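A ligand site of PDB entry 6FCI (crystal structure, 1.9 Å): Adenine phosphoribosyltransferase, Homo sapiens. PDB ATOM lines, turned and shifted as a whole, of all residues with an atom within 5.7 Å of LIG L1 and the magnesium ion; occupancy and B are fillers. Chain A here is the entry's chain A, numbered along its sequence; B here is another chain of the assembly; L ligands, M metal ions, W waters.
O3 of LIG L1 sits close to OD2 of Asp 126 (2.4 Å).
The side-chain hydroxyl (OH) of Tyr 104 is in hydrogen-bond range of an oxygen (O10) of LIG L1, at 2.5 Å.
O6 of LIG L1 sits at hydrogen-bond distance from N of Thr 131, at 2.9 Å.
The side-chain hydroxyl (OG1) of Thr 131 sits at hydrogen-bond distance from an oxygen (O6) of LIG L1 (2.5 Å).
An oxygen (O7) of LIG L1 sits at hydrogen-bond distance from the backbone NH of Thr 134 (2.9 Å).
The side-chain hydroxyl (OG1) of Thr 134 lies within hydrogen-bond range of an oxygen (O7) of LIG L1 (2.6 Å).
The backbone NH (N) of Arg 66 sits close to an oxygen (O14) of LIG L1, at 3.1 Å.
An oxygen (O13) of LIG L1 lies within salt-bridge range of the guanidinium group (NE) of Arg 66 (2.7 Å).
OD1 of Asp 127 lies close to O2 of LIG L1 (2.7 Å).
The backbone NH (N) of Ala 130 lies within hydrogen-bond range of an oxygen (O8) of LIG L1 (2.7 Å).
An oxygen (O12) of LIG L1 lies within salt-bridge range of the guanidinium group of Arg 86 of chain B (2.8 Å).
N of Glu 103 is in hydrogen-bond range of O6 of LIG L1 (2.8 Å).
The backbone NH (N) of Gly 132 sits at hydrogen-bond distance from an oxygen (O8) of LIG L1.
An oxygen (O14) of LIG L1 sits close to the backbone NH of Ser 65 (3.0 Å).
NZ of Lys 90 of chain B lies within salt-bridge range of O10 of LIG L1 (3.1 Å).
The side-chain amino group (NZ) of Lys 87 lies within salt-bridge range of an oxygen (O9) of LIG L1 (3.5 Å).
The side-chain hydroxyl (OH) of Tyr 104 is in hydrogen-bond range of a nitrogen (N1) of LG2 L2 (3.4 Å).
The guanidinium group of Arg 66 is in hydrogen-bond range of a nitrogen (N5) of LG2 L2 (2.9 Å).
A nitrogen (N2) of LG2 L2 is in hydrogen-bond range of the side-chain carboxylate of Glu 103, at 2.6 Å.
The magnesium ion is bound by an oxygen (O14) of LIG L1, water W3, water W1, an oxygen (O2) of LIG L1, an oxygen (O1) of LIG L1 and an oxygen (O3) of LIG L1.
The side-chain carboxylate (OD1) of Asp 126 lies within hydrogen-bond range of the backbone NH (N) of Gly 67 (3.2 Å).
The side-chain hydroxyl of Tyr 104 sits at hydrogen-bond distance from the guanidinium group of Arg 66 (2.9 Å).
The side-chain hydroxyl of Thr 131 sits close to the backbone NH of Gly 133.
The guanidinium group of Arg 66 lies within salt-bridge range of the side-chain carboxylate of Asp 127.
The guanidinium group (NE) of Arg 86 of chain B lies within salt-bridge range of the side-chain carboxylate (OD2) of Asp 64 of chain B.
The side-chain amino group of Lys 87 sits at hydrogen-bond distance from the backbone carbonyl oxygen of Asp 64 of chain A (2.9 Å).
O4 of LIG L1 sits at hydrogen-bond distance from N1 of LG2 L2, at 3.1 Å.
C of Asp 64 of chain A touches O14 of LIG L1, at 3.9 Å.
Leu 102 touches LIG L1.
Leu 128 touches LIG L1 (O to C5, 3.5 Å).
Leu 129 touches LIG L1.
Gly 133 touches LIG L1.
Hydrophobic or aromatic side chains within 4 Å of LIG L1: Leu 102, Tyr 104 and Ala 130.
Water W1 lies within hydrogen-bond range of O of Asp 64 of chain A, NZ of Lys 87 and O11 of LIG L1.
Water W4 lies within hydrogen-bond range of NZ of Lys 87 (2.6 Å), O12 of LIG L1 (2.6 Å) and OG of Ser 65 (3.4 Å).
Water W5 lies within hydrogen-bond range of the side-chain hydroxyl of Tyr 100 (2.7 Å), an oxygen (O9) of LIG L1 (2.7 Å) and the side-chain hydroxyl of Thr 134 (2.8 Å).
Water W6 lies within hydrogen-bond range of O8 of LIG L1 (2.8 Å), N of Met 135 (2.9 Å) and N of Thr 134 (3.4 Å).
O of Asp 64 of chain A touches the magnesium ion (3.8 Å).
Ser 65 touches the magnesium ion (N to MG, 3.99 Å).
Of the 25 residues printed, 2 come within 4 Å of the magnesium ion.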
ATOM      1  N   LEU A  63      20.796 -11.063  26.289  1.00  0.00           N
ATOM      2  CA  LEU A  63      21.269  -9.758  25.848  1.00  0.00           C
ATOM      3  C   LEU A  63      21.456  -9.669  24.332  1.00  0.00           C
ATOM      4  O   LEU A  63      22.271 -10.397  23.738  1.00  0.00           O
ATOM      5  CB  LEU A  63      22.581  -9.380  26.552  1.00  0.00           C
ATOM      6  CG  LEU A  63      22.533  -9.355  28.081  1.00  0.00           C
ATOM      7  CD1 LEU A  63      23.810  -8.765  28.646  1.00  0.00           C
ATOM      8  CD2 LEU A  63      21.321  -8.580  28.600  1.00  0.00           C
ATOM      9  N   ASP A  64      20.673  -8.795  23.716  1.00  0.00           N
ATOM     10  CA  ASP A  64      20.824  -8.389  22.304  1.00  0.00           C
ATOM     11  C   ASP A  64      22.282  -8.122  21.984  1.00  0.00           C
ATOM     12  O   ASP A  64      22.919  -7.324  22.678  1.00  0.00           O
ATOM     13  CB  ASP A  64      20.012  -7.101  22.114  1.00  0.00           C
ATOM     14  CG  ASP A  64      19.786  -6.745  20.661  1.00  0.00           C
ATOM     15  OD1 ASP A  64      20.255  -7.478  19.765  1.00  0.00           O
ATOM     16  OD2 ASP A  64      19.100  -5.720  20.415  1.00  0.00           O
ATOM     17  N   SER A  65      22.840  -8.750  20.946  1.00  0.00           N
ATOM     18  CA  SER A  65      22.120  -9.704  20.105  1.00  0.00           C
ATOM     19  C   SER A  65      22.635 -11.119  20.317  1.00  0.00           C
ATOM     20  O   SER A  65      21.874 -12.082  20.262  1.00  0.00           O
ATOM     21  CB  SER A  65      22.282  -9.332  18.624  1.00  0.00           C
ATOM     22  OG  SER A  65      21.510  -8.195  18.279  1.00  0.00           O
ATOM     23  N   ARG A  66      23.944 -11.253  20.506  1.00  0.00           N
ATOM     24  CA  ARG A  66      24.570 -12.573  20.549  1.00  0.00           C
ATOM     25  C   ARG A  66      24.125 -13.368  21.770  1.00  0.00           C
ATOM     26  O   ARG A  66      24.124 -14.591  21.747  1.00  0.00           O
ATOM     27  CB  ARG A  66      26.097 -12.446  20.515  1.00  0.00           C
ATOM     28  CG  ARG A  66      26.641 -12.203  19.123  1.00  0.00           C
ATOM     29  CD  ARG A  66      28.155 -12.228  19.101  1.00  0.00           C
ATOM     30  NE  ARG A  66      28.709 -10.891  19.215  1.00  0.00           N
ATOM     31  CZ  ARG A  66      29.909 -10.630  19.723  1.00  0.00           C
ATOM     32  NH1 ARG A  66      30.667 -11.607  20.197  1.00  0.00           N
ATOM     33  NH2 ARG A  66      30.351  -9.382  19.758  1.00  0.00           N
ATOM     34  N   GLY A  67      23.668 -12.661  22.805  1.00  0.00           N
ATOM     35  CA  GLY A  67      23.021 -13.311  23.948  1.00  0.00           C
ATOM     36  C   GLY A  67      21.710 -13.977  23.567  1.00  0.00           C
ATOM     37  O   GLY A  67      21.273 -14.936  24.224  1.00  0.00           O
ATOM     38  N   LYS A  87      19.248  -3.510  22.405  1.00  0.00           N
ATOM     39  CA  LYS A  87      19.867  -2.233  22.060  1.00  0.00           C
ATOM     40  C   LYS A  87      18.792  -1.169  21.901  1.00  0.00           C
ATOM     41  O   LYS A  87      17.700  -1.431  21.368  1.00  0.00           O
ATOM     42  CB  LYS A  87      20.689  -2.369  20.767  1.00  0.00           C
ATOM     43  CG  LYS A  87      21.801  -3.406  20.817  1.00  0.00           C
ATOM     44  CD  LYS A  87      23.010  -2.912  21.603  1.00  0.00           C
ATOM     45  CE  LYS A  87      24.289  -3.627  21.200  1.00  0.00           C
ATOM     46  NZ  LYS A  87      24.263  -5.086  21.504  1.00  0.00           N
ATOM     47  N   TYR A 100      26.296   2.752  28.256  1.00  0.00           N
ATOM     48  CA  TYR A 100      27.417   1.961  28.741  1.00  0.00           C
ATOM     49  C   TYR A 100      28.473   1.874  27.659  1.00  0.00           C
ATOM     50  O   TYR A 100      28.234   2.201  26.496  1.00  0.00           O
ATOM     51  CB  TYR A 100      26.950   0.550  29.125  1.00  0.00           C
ATOM     52  CG  TYR A 100      26.537  -0.294  27.936  1.00  0.00           C
ATOM     53  CD1 TYR A 100      25.239  -0.252  27.452  1.00  0.00           C
ATOM     54  CD2 TYR A 100      27.436  -1.151  27.314  1.00  0.00           C
ATOM     55  CE1 TYR A 100      24.851  -1.031  26.380  1.00  0.00           C
ATOM     56  CE2 TYR A 100      27.057  -1.941  26.239  1.00  0.00           C
ATOM     57  CZ  TYR A 100      25.758  -1.882  25.788  1.00  0.00           C
ATOM     58  OH  TYR A 100      25.360  -2.649  24.709  1.00  0.00           O
ATOM     59  N   SER A 101      29.656   1.441  28.044  1.00  0.00           N
ATOM     60  CA  SER A 101      30.688   1.121  27.081  1.00  0.00           C
ATOM     61  C   SER A 101      30.999  -0.373  27.134  1.00  0.00           C
ATOM     62  O   SER A 101      30.844  -1.022  28.171  1.00  0.00           O
ATOM     63  CB  SER A 101      31.946   1.937  27.360  1.00  0.00           C
ATOM     64  OG  SER A 101      32.569   1.528  28.556  1.00  0.00           O
ATOM     65  N   LEU A 102      31.383  -0.906  25.984  1.00  0.00           N
ATOM     66  CA  LEU A 102      31.877  -2.265  25.888  1.00  0.00           C
ATOM     67  C   LEU A 102      33.320  -2.181  25.411  1.00  0.00           C
ATOM     68  O   LEU A 102      33.873  -1.082  25.285  1.00  0.00           O
ATOM     69  CB  LEU A 102      31.031  -3.076  24.899  1.00  0.00           C
ATOM     70  CG  LEU A 102      30.961  -2.489  23.482  1.00  0.00           C
ATOM     71  CD1 LEU A 102      30.843  -3.612  22.465  1.00  0.00           C
ATOM     72  CD2 LEU A 102      29.812  -1.510  23.351  1.00  0.00           C
ATOM     73  N   GLU A 103      33.932  -3.322  25.120  1.00  0.00           N
ATOM     74  CA  GLU A 103      35.358  -3.348  24.829  1.00  0.00           C
ATOM     75  C   GLU A 103      35.742  -2.411  23.684  1.00  0.00           C
ATOM     76  O   GLU A 103      36.773  -1.756  23.736  1.00  0.00           O
ATOM     77  CB  GLU A 103      35.829  -4.770  24.501  1.00  0.00           C
ATOM     78  CG  GLU A 103      37.345  -4.847  24.296  1.00  0.00           C
ATOM     79  CD  GLU A 103      37.822  -6.221  23.890  1.00  0.00           C
ATOM     80  OE1 GLU A 103      36.997  -7.149  23.772  1.00  0.00           O
ATOM     81  OE2 GLU A 103      39.048  -6.383  23.680  1.00  0.00           O
ATOM     82  N   TYR A 104      34.923  -2.379  22.638  1.00  0.00           N
ATOM     83  CA  TYR A 104      35.305  -1.677  21.410  1.00  0.00           C
ATOM     84  C   TYR A 104      34.290  -0.629  20.955  1.00  0.00           C
ATOM     85  O   TYR A 104      34.201  -0.309  19.776  1.00  0.00           O
ATOM     86  CB  TYR A 104      35.582  -2.673  20.264  1.00  0.00           C
ATOM     87  CG  TYR A 104      34.546  -3.763  20.112  1.00  0.00           C
ATOM     88  CD1 TYR A 104      33.275  -3.482  19.643  1.00  0.00           C
ATOM     89  CD2 TYR A 104      34.876  -5.090  20.380  1.00  0.00           C
ATOM     90  CE1 TYR A 104      32.331  -4.483  19.492  1.00  0.00           C
ATOM     91  CE2 TYR A 104      33.948  -6.101  20.213  1.00  0.00           C
ATOM     92  CZ  TYR A 104      32.678  -5.794  19.780  1.00  0.00           C
ATOM     93  OH  TYR A 104      31.750  -6.795  19.614  1.00  0.00           O
ATOM     94  N   ALA A 107      27.335   2.049  23.681  1.00  0.00           N
ATOM     95  CA  ALA A 107      25.984   1.748  23.246  1.00  0.00           C
ATOM     96  C   ALA A 107      24.986   2.059  24.345  1.00  0.00           C
ATOM     97  O   ALA A 107      25.356   2.578  25.407  1.00  0.00           O
ATOM     98  CB  ALA A 107      25.874   0.285  22.843  1.00  0.00           C
ATOM     99  N   ASP A 126      24.790 -13.880  28.406  1.00  0.00           N
ATOM    100  CA  ASP A 126      25.340 -13.301  27.194  1.00  0.00           C
ATOM    101  C   ASP A 126      26.427 -14.231  26.652  1.00  0.00           C
ATOM    102  O   ASP A 126      26.860 -15.159  27.334  1.00  0.00           O
ATOM    103  CB  ASP A 126      25.922 -11.916  27.484  1.00  0.00           C
ATOM    104  CG  ASP A 126      25.912 -11.024  26.271  1.00  0.00           C
ATOM    105  OD1 ASP A 126      25.408 -11.445  25.213  1.00  0.00           O
ATOM    106  OD2 ASP A 126      26.405  -9.882  26.383  1.00  0.00           O
ATOM    107  N   ASP A 127      26.832 -14.007  25.414  1.00  0.00           N
ATOM    108  CA  ASP A 127      27.794 -14.889  24.764  1.00  0.00           C
ATOM    109  C   ASP A 127      29.193 -14.713  25.358  1.00  0.00           C
ATOM    110  O   ASP A 127      29.897 -15.690  25.616  1.00  0.00           O
ATOM    111  CB  ASP A 127      27.817 -14.668  23.244  1.00  0.00           C
ATOM    112  CG  ASP A 127      28.427 -13.343  22.845  1.00  0.00           C
ATOM    113  OD1 ASP A 127      28.078 -12.310  23.443  1.00  0.00           O
ATOM    114  OD2 ASP A 127      29.234 -13.332  21.887  1.00  0.00           O
ATOM    115  N   LEU A 128      29.581 -13.469  25.592  1.00  0.00           N
ATOM    116  CA  LEU A 128      30.947 -13.172  26.044  1.00  0.00           C
ATOM    117  C   LEU A 128      30.949 -12.033  27.050  1.00  0.00           C
ATOM    118  O   LEU A 128      30.209 -11.052  26.894  1.00  0.00           O
ATOM    119  CB  LEU A 128      31.835 -12.839  24.831  1.00  0.00           C
ATOM    120  CG  LEU A 128      33.331 -12.646  25.062  1.00  0.00           C
ATOM    121  CD1 LEU A 128      34.120 -13.217  23.894  1.00  0.00           C
ATOM    122  CD2 LEU A 128      33.656 -11.165  25.240  1.00  0.00           C
ATOM    123  N   LEU A 129      31.738 -12.185  28.107  1.00  0.00           N
ATOM    124  CA  LEU A 129      32.072 -11.076  28.999  1.00  0.00           C
ATOM    125  C   LEU A 129      33.458 -10.518  28.694  1.00  0.00           C
ATOM    126  O   LEU A 129      34.445 -11.246  28.660  1.00  0.00           O
ATOM    127  CB  LEU A 129      32.023 -11.521  30.463  1.00  0.00           C
ATOM    128  CG  LEU A 129      32.327 -10.412  31.487  1.00  0.00           C
ATOM    129  CD1 LEU A 129      31.114  -9.545  31.718  1.00  0.00           C
ATOM    130  CD2 LEU A 129      32.815 -10.999  32.794  1.00  0.00           C
ATOM    131  N   ALA A 130      33.532  -9.206  28.472  1.00  0.00           N
ATOM    132  CA  ALA A 130      34.814  -8.530  28.323  1.00  0.00           C
ATOM    133  C   ALA A 130      35.018  -7.499  29.432  1.00  0.00           C
ATOM    134  O   ALA A 130      35.435  -7.851  30.529  1.00  0.00           O
ATOM    135  CB  ALA A 130      34.925  -7.879  26.944  1.00  0.00           C
ATOM    136  N   THR A 131      34.740  -6.227  29.144  1.00  0.00           N
ATOM    137  CA  THR A 131      34.852  -5.186  30.172  1.00  0.00           C
ATOM    138  C   THR A 131      33.745  -5.311  31.217  1.00  0.00           C
ATOM    139  O   THR A 131      33.856  -4.773  32.311  1.00  0.00           O
ATOM    140  CB  THR A 131      34.816  -3.750  29.590  1.00  0.00           C
ATOM    141  OG1 THR A 131      33.515  -3.478  29.045  1.00  0.00           O
ATOM    142  CG2 THR A 131      35.869  -3.564  28.514  1.00  0.00           C
ATOM    143  N   GLY A 132      32.664  -5.997  30.851  1.00  0.00           N
ATOM    144  CA  GLY A 132      31.515  -6.162  31.744  1.00  0.00           C
ATOM    145  C   GLY A 132      30.539  -5.000  31.690  1.00  0.00           C
ATOM    146  O   GLY A 132      29.564  -4.949  32.447  1.00  0.00           O
ATOM    147  N   GLY A 133      30.787  -4.062  30.785  1.00  0.00           N
ATOM    148  CA  GLY A 133      29.925  -2.885  30.643  1.00  0.00           C
ATOM    149  C   GLY A 133      28.522  -3.269  30.198  1.00  0.00           C
ATOM    150  O   GLY A 133      27.533  -2.777  30.729  1.00  0.00           O
ATOM    151  N   THR A 134      28.439  -4.190  29.241  1.00  0.00           N
ATOM    152  CA  THR A 134      27.156  -4.611  28.711  1.00  0.00           C
ATOM    153  C   THR A 134      26.319  -5.320  29.777  1.00  0.00           C
ATOM    154  O   THR A 134      25.136  -5.027  29.943  1.00  0.00           O
ATOM    155  CB  THR A 134      27.328  -5.546  27.494  1.00  0.00           C
ATOM    156  OG1 THR A 134      28.083  -4.873  26.484  1.00  0.00           O
ATOM    157  CG2 THR A 134      25.966  -5.953  26.933  1.00  0.00           C
ATOM    158  N   MET A 135      26.950  -6.237  30.507  1.00  0.00           N
ATOM    159  CA  MET A 135      26.257  -6.981  31.544  1.00  0.00           C
ATOM    160  C   MET A 135      25.851  -6.061  32.700  1.00  0.00           C
ATOM    161  O   MET A 135      24.764  -6.197  33.251  1.00  0.00           O
ATOM    162  CB  MET A 135      27.124  -8.129  32.062  1.00  0.00           C
ATOM    163  CG  MET A 135      26.368  -9.139  32.912  1.00  0.00           C
ATOM    164  SD  MET A 135      25.496 -10.375  31.944  1.00  0.00           S
ATOM    165  CE  MET A 135      26.851 -11.470  31.503  1.00  0.00           C
ATOM    166  N   ASP B  64      19.929 -12.193  12.237  1.00  0.00           N
ATOM    167  CA  ASP B  64      20.219 -11.161  13.233  1.00  0.00           C
ATOM    168  C   ASP B  64      19.114 -10.112  13.163  1.00  0.00           C
ATOM    169  O   ASP B  64      18.837  -9.616  12.073  1.00  0.00           O
ATOM    170  CB  ASP B  64      21.552 -10.505  12.840  1.00  0.00           C
ATOM    171  CG  ASP B  64      22.122  -9.620  13.935  1.00  0.00           C
ATOM    172  OD1 ASP B  64      21.494  -9.474  15.007  1.00  0.00           O
ATOM    173  OD2 ASP B  64      23.210  -9.043  13.714  1.00  0.00           O
ATOM    174  N   ARG B  86      24.195 -11.889   9.802  1.00  0.00           N
ATOM    175  CA  ARG B  86      24.255 -10.762  10.752  1.00  0.00           C
ATOM    176  C   ARG B  86      24.115  -9.411  10.037  1.00  0.00           C
ATOM    177  O   ARG B  86      24.306  -9.314   8.823  1.00  0.00           O
ATOM    178  CB  ARG B  86      25.566 -10.797  11.534  1.00  0.00           C
ATOM    179  CG  ARG B  86      25.708 -11.981  12.479  1.00  0.00           C
ATOM    180  CD  ARG B  86      26.294 -11.571  13.827  1.00  0.00           C
ATOM    181  NE  ARG B  86      25.459 -10.574  14.484  1.00  0.00           N
ATOM    182  CZ  ARG B  86      25.775  -9.944  15.615  1.00  0.00           C
ATOM    183  NH1 ARG B  86      26.911 -10.226  16.250  1.00  0.00           N
ATOM    184  NH2 ARG B  86      24.953  -9.033  16.111  1.00  0.00           N
ATOM    185  N   LYS B  90      29.313  -6.782  11.764  1.00  0.00           N
ATOM    186  CA  LYS B  90      29.306  -7.496  13.047  1.00  0.00           C
ATOM    187  C   LYS B  90      30.132  -8.786  13.047  1.00  0.00           C
ATOM    188  O   LYS B  90      30.590  -9.240  14.100  1.00  0.00           O
ATOM    189  CB  LYS B  90      27.861  -7.797  13.474  1.00  0.00           C
ATOM    190  CG  LYS B  90      27.017  -6.561  13.710  1.00  0.00           C
ATOM    191  CD  LYS B  90      27.013  -6.119  15.171  1.00  0.00           C
ATOM    192  CE  LYS B  90      28.413  -5.938  15.724  1.00  0.00           C
ATOM    193  NZ  LYS B  90      28.413  -5.389  17.116  1.00  0.00           N
HETATM  194  C1  LIG L   1      29.438  -7.746  22.491  1.00  0.00           C
HETATM  195  C2  LIG L   1      29.227  -9.123  23.099  1.00  0.00           C
HETATM  196  C3  LIG L   1      28.830  -8.800  24.523  1.00  0.00           C
HETATM  197  C4  LIG L   1      29.574  -7.508  24.835  1.00  0.00           C
HETATM  198  C5  LIG L   1      30.792  -7.806  25.718  1.00  0.00           C
HETATM  199  O1  LIG L   1      28.184  -7.274  22.014  1.00  0.00           O
HETATM  200  O2  LIG L   1      28.213  -9.853  22.400  1.00  0.00           O
HETATM  201  O3  LIG L   1      27.408  -8.579  24.591  1.00  0.00           O
HETATM  202  O4  LIG L   1      29.944  -6.942  23.570  1.00  0.00           O
HETATM  203  O5  LIG L   1      31.625  -6.660  25.863  1.00  0.00           O
HETATM  204  P1  LIG L   1      31.779  -5.899  27.290  1.00  0.00           P
HETATM  205  O6  LIG L   1      33.030  -5.076  27.126  1.00  0.00           O
HETATM  206  O7  LIG L   1      30.527  -5.067  27.422  1.00  0.00           O
HETATM  207  O8  LIG L   1      31.900  -7.015  28.290  1.00  0.00           O
HETATM  208  P2  LIG L   1      28.070  -6.198  20.809  1.00  0.00           P
HETATM  209  O9  LIG L   1      27.797  -4.851  21.422  1.00  0.00           O
HETATM  210  O10 LIG L   1      29.262  -6.371  19.890  1.00  0.00           O
HETATM  211  O11 LIG L   1      26.712  -6.591  20.010  1.00  0.00           O
HETATM  212  P3  LIG L   1      26.286  -8.034  19.416  1.00  0.00           P
HETATM  213  O12 LIG L   1      25.158  -7.662  18.491  1.00  0.00           O
HETATM  214  O13 LIG L   1      27.515  -8.557  18.699  1.00  0.00           O
HETATM  215  O14 LIG L   1      25.863  -8.849  20.608  1.00  0.00           O
HETATM  216  N1  LG2 L   2      32.504  -8.421  22.551  1.00  0.00           N
HETATM  217  C1  LG2 L   2      33.286  -7.594  23.277  1.00  0.00           C
HETATM  218  N2  LG2 L   2      34.590  -7.937  23.158  1.00  0.00           N
HETATM  219  C2  LG2 L   2      34.665  -9.005  22.351  1.00  0.00           C
HETATM  220  C3  LG2 L   2      35.713  -9.840  21.821  1.00  0.00           C
HETATM  221  N3  LG2 L   2      37.026  -9.574  22.157  1.00  0.00           N
HETATM  222  N4  LG2 L   2      35.378 -10.872  20.971  1.00  0.00           N
HETATM  223  C4  LG2 L   2      34.091 -11.111  20.643  1.00  0.00           C
HETATM  224  N5  LG2 L   2      33.071 -10.376  21.121  1.00  0.00           N
HETATM  225  C5  LG2 L   2      33.353  -9.325  21.955  1.00  0.00           C
HETATM  226 MG    MG M   1      26.501  -8.639  22.528  1.00  0.00          MG
HETATM  227  O   HOH W   1      25.383  -6.929  23.017  1.00  0.00           O
HETATM  228  O   HOH W   2      28.011  -2.464  19.894  1.00  0.00           O
HETATM  229  O   HOH W   3      24.966  -9.911  23.143  1.00  0.00           O
HETATM  230  O   HOH W   4      23.633  -5.614  19.041  1.00  0.00           O
HETATM  231  O   HOH W   5      26.845  -4.754  23.985  1.00  0.00           O
HETATM  232  O   HOH W   6      29.442  -7.392  29.663  1.00  0.00           O
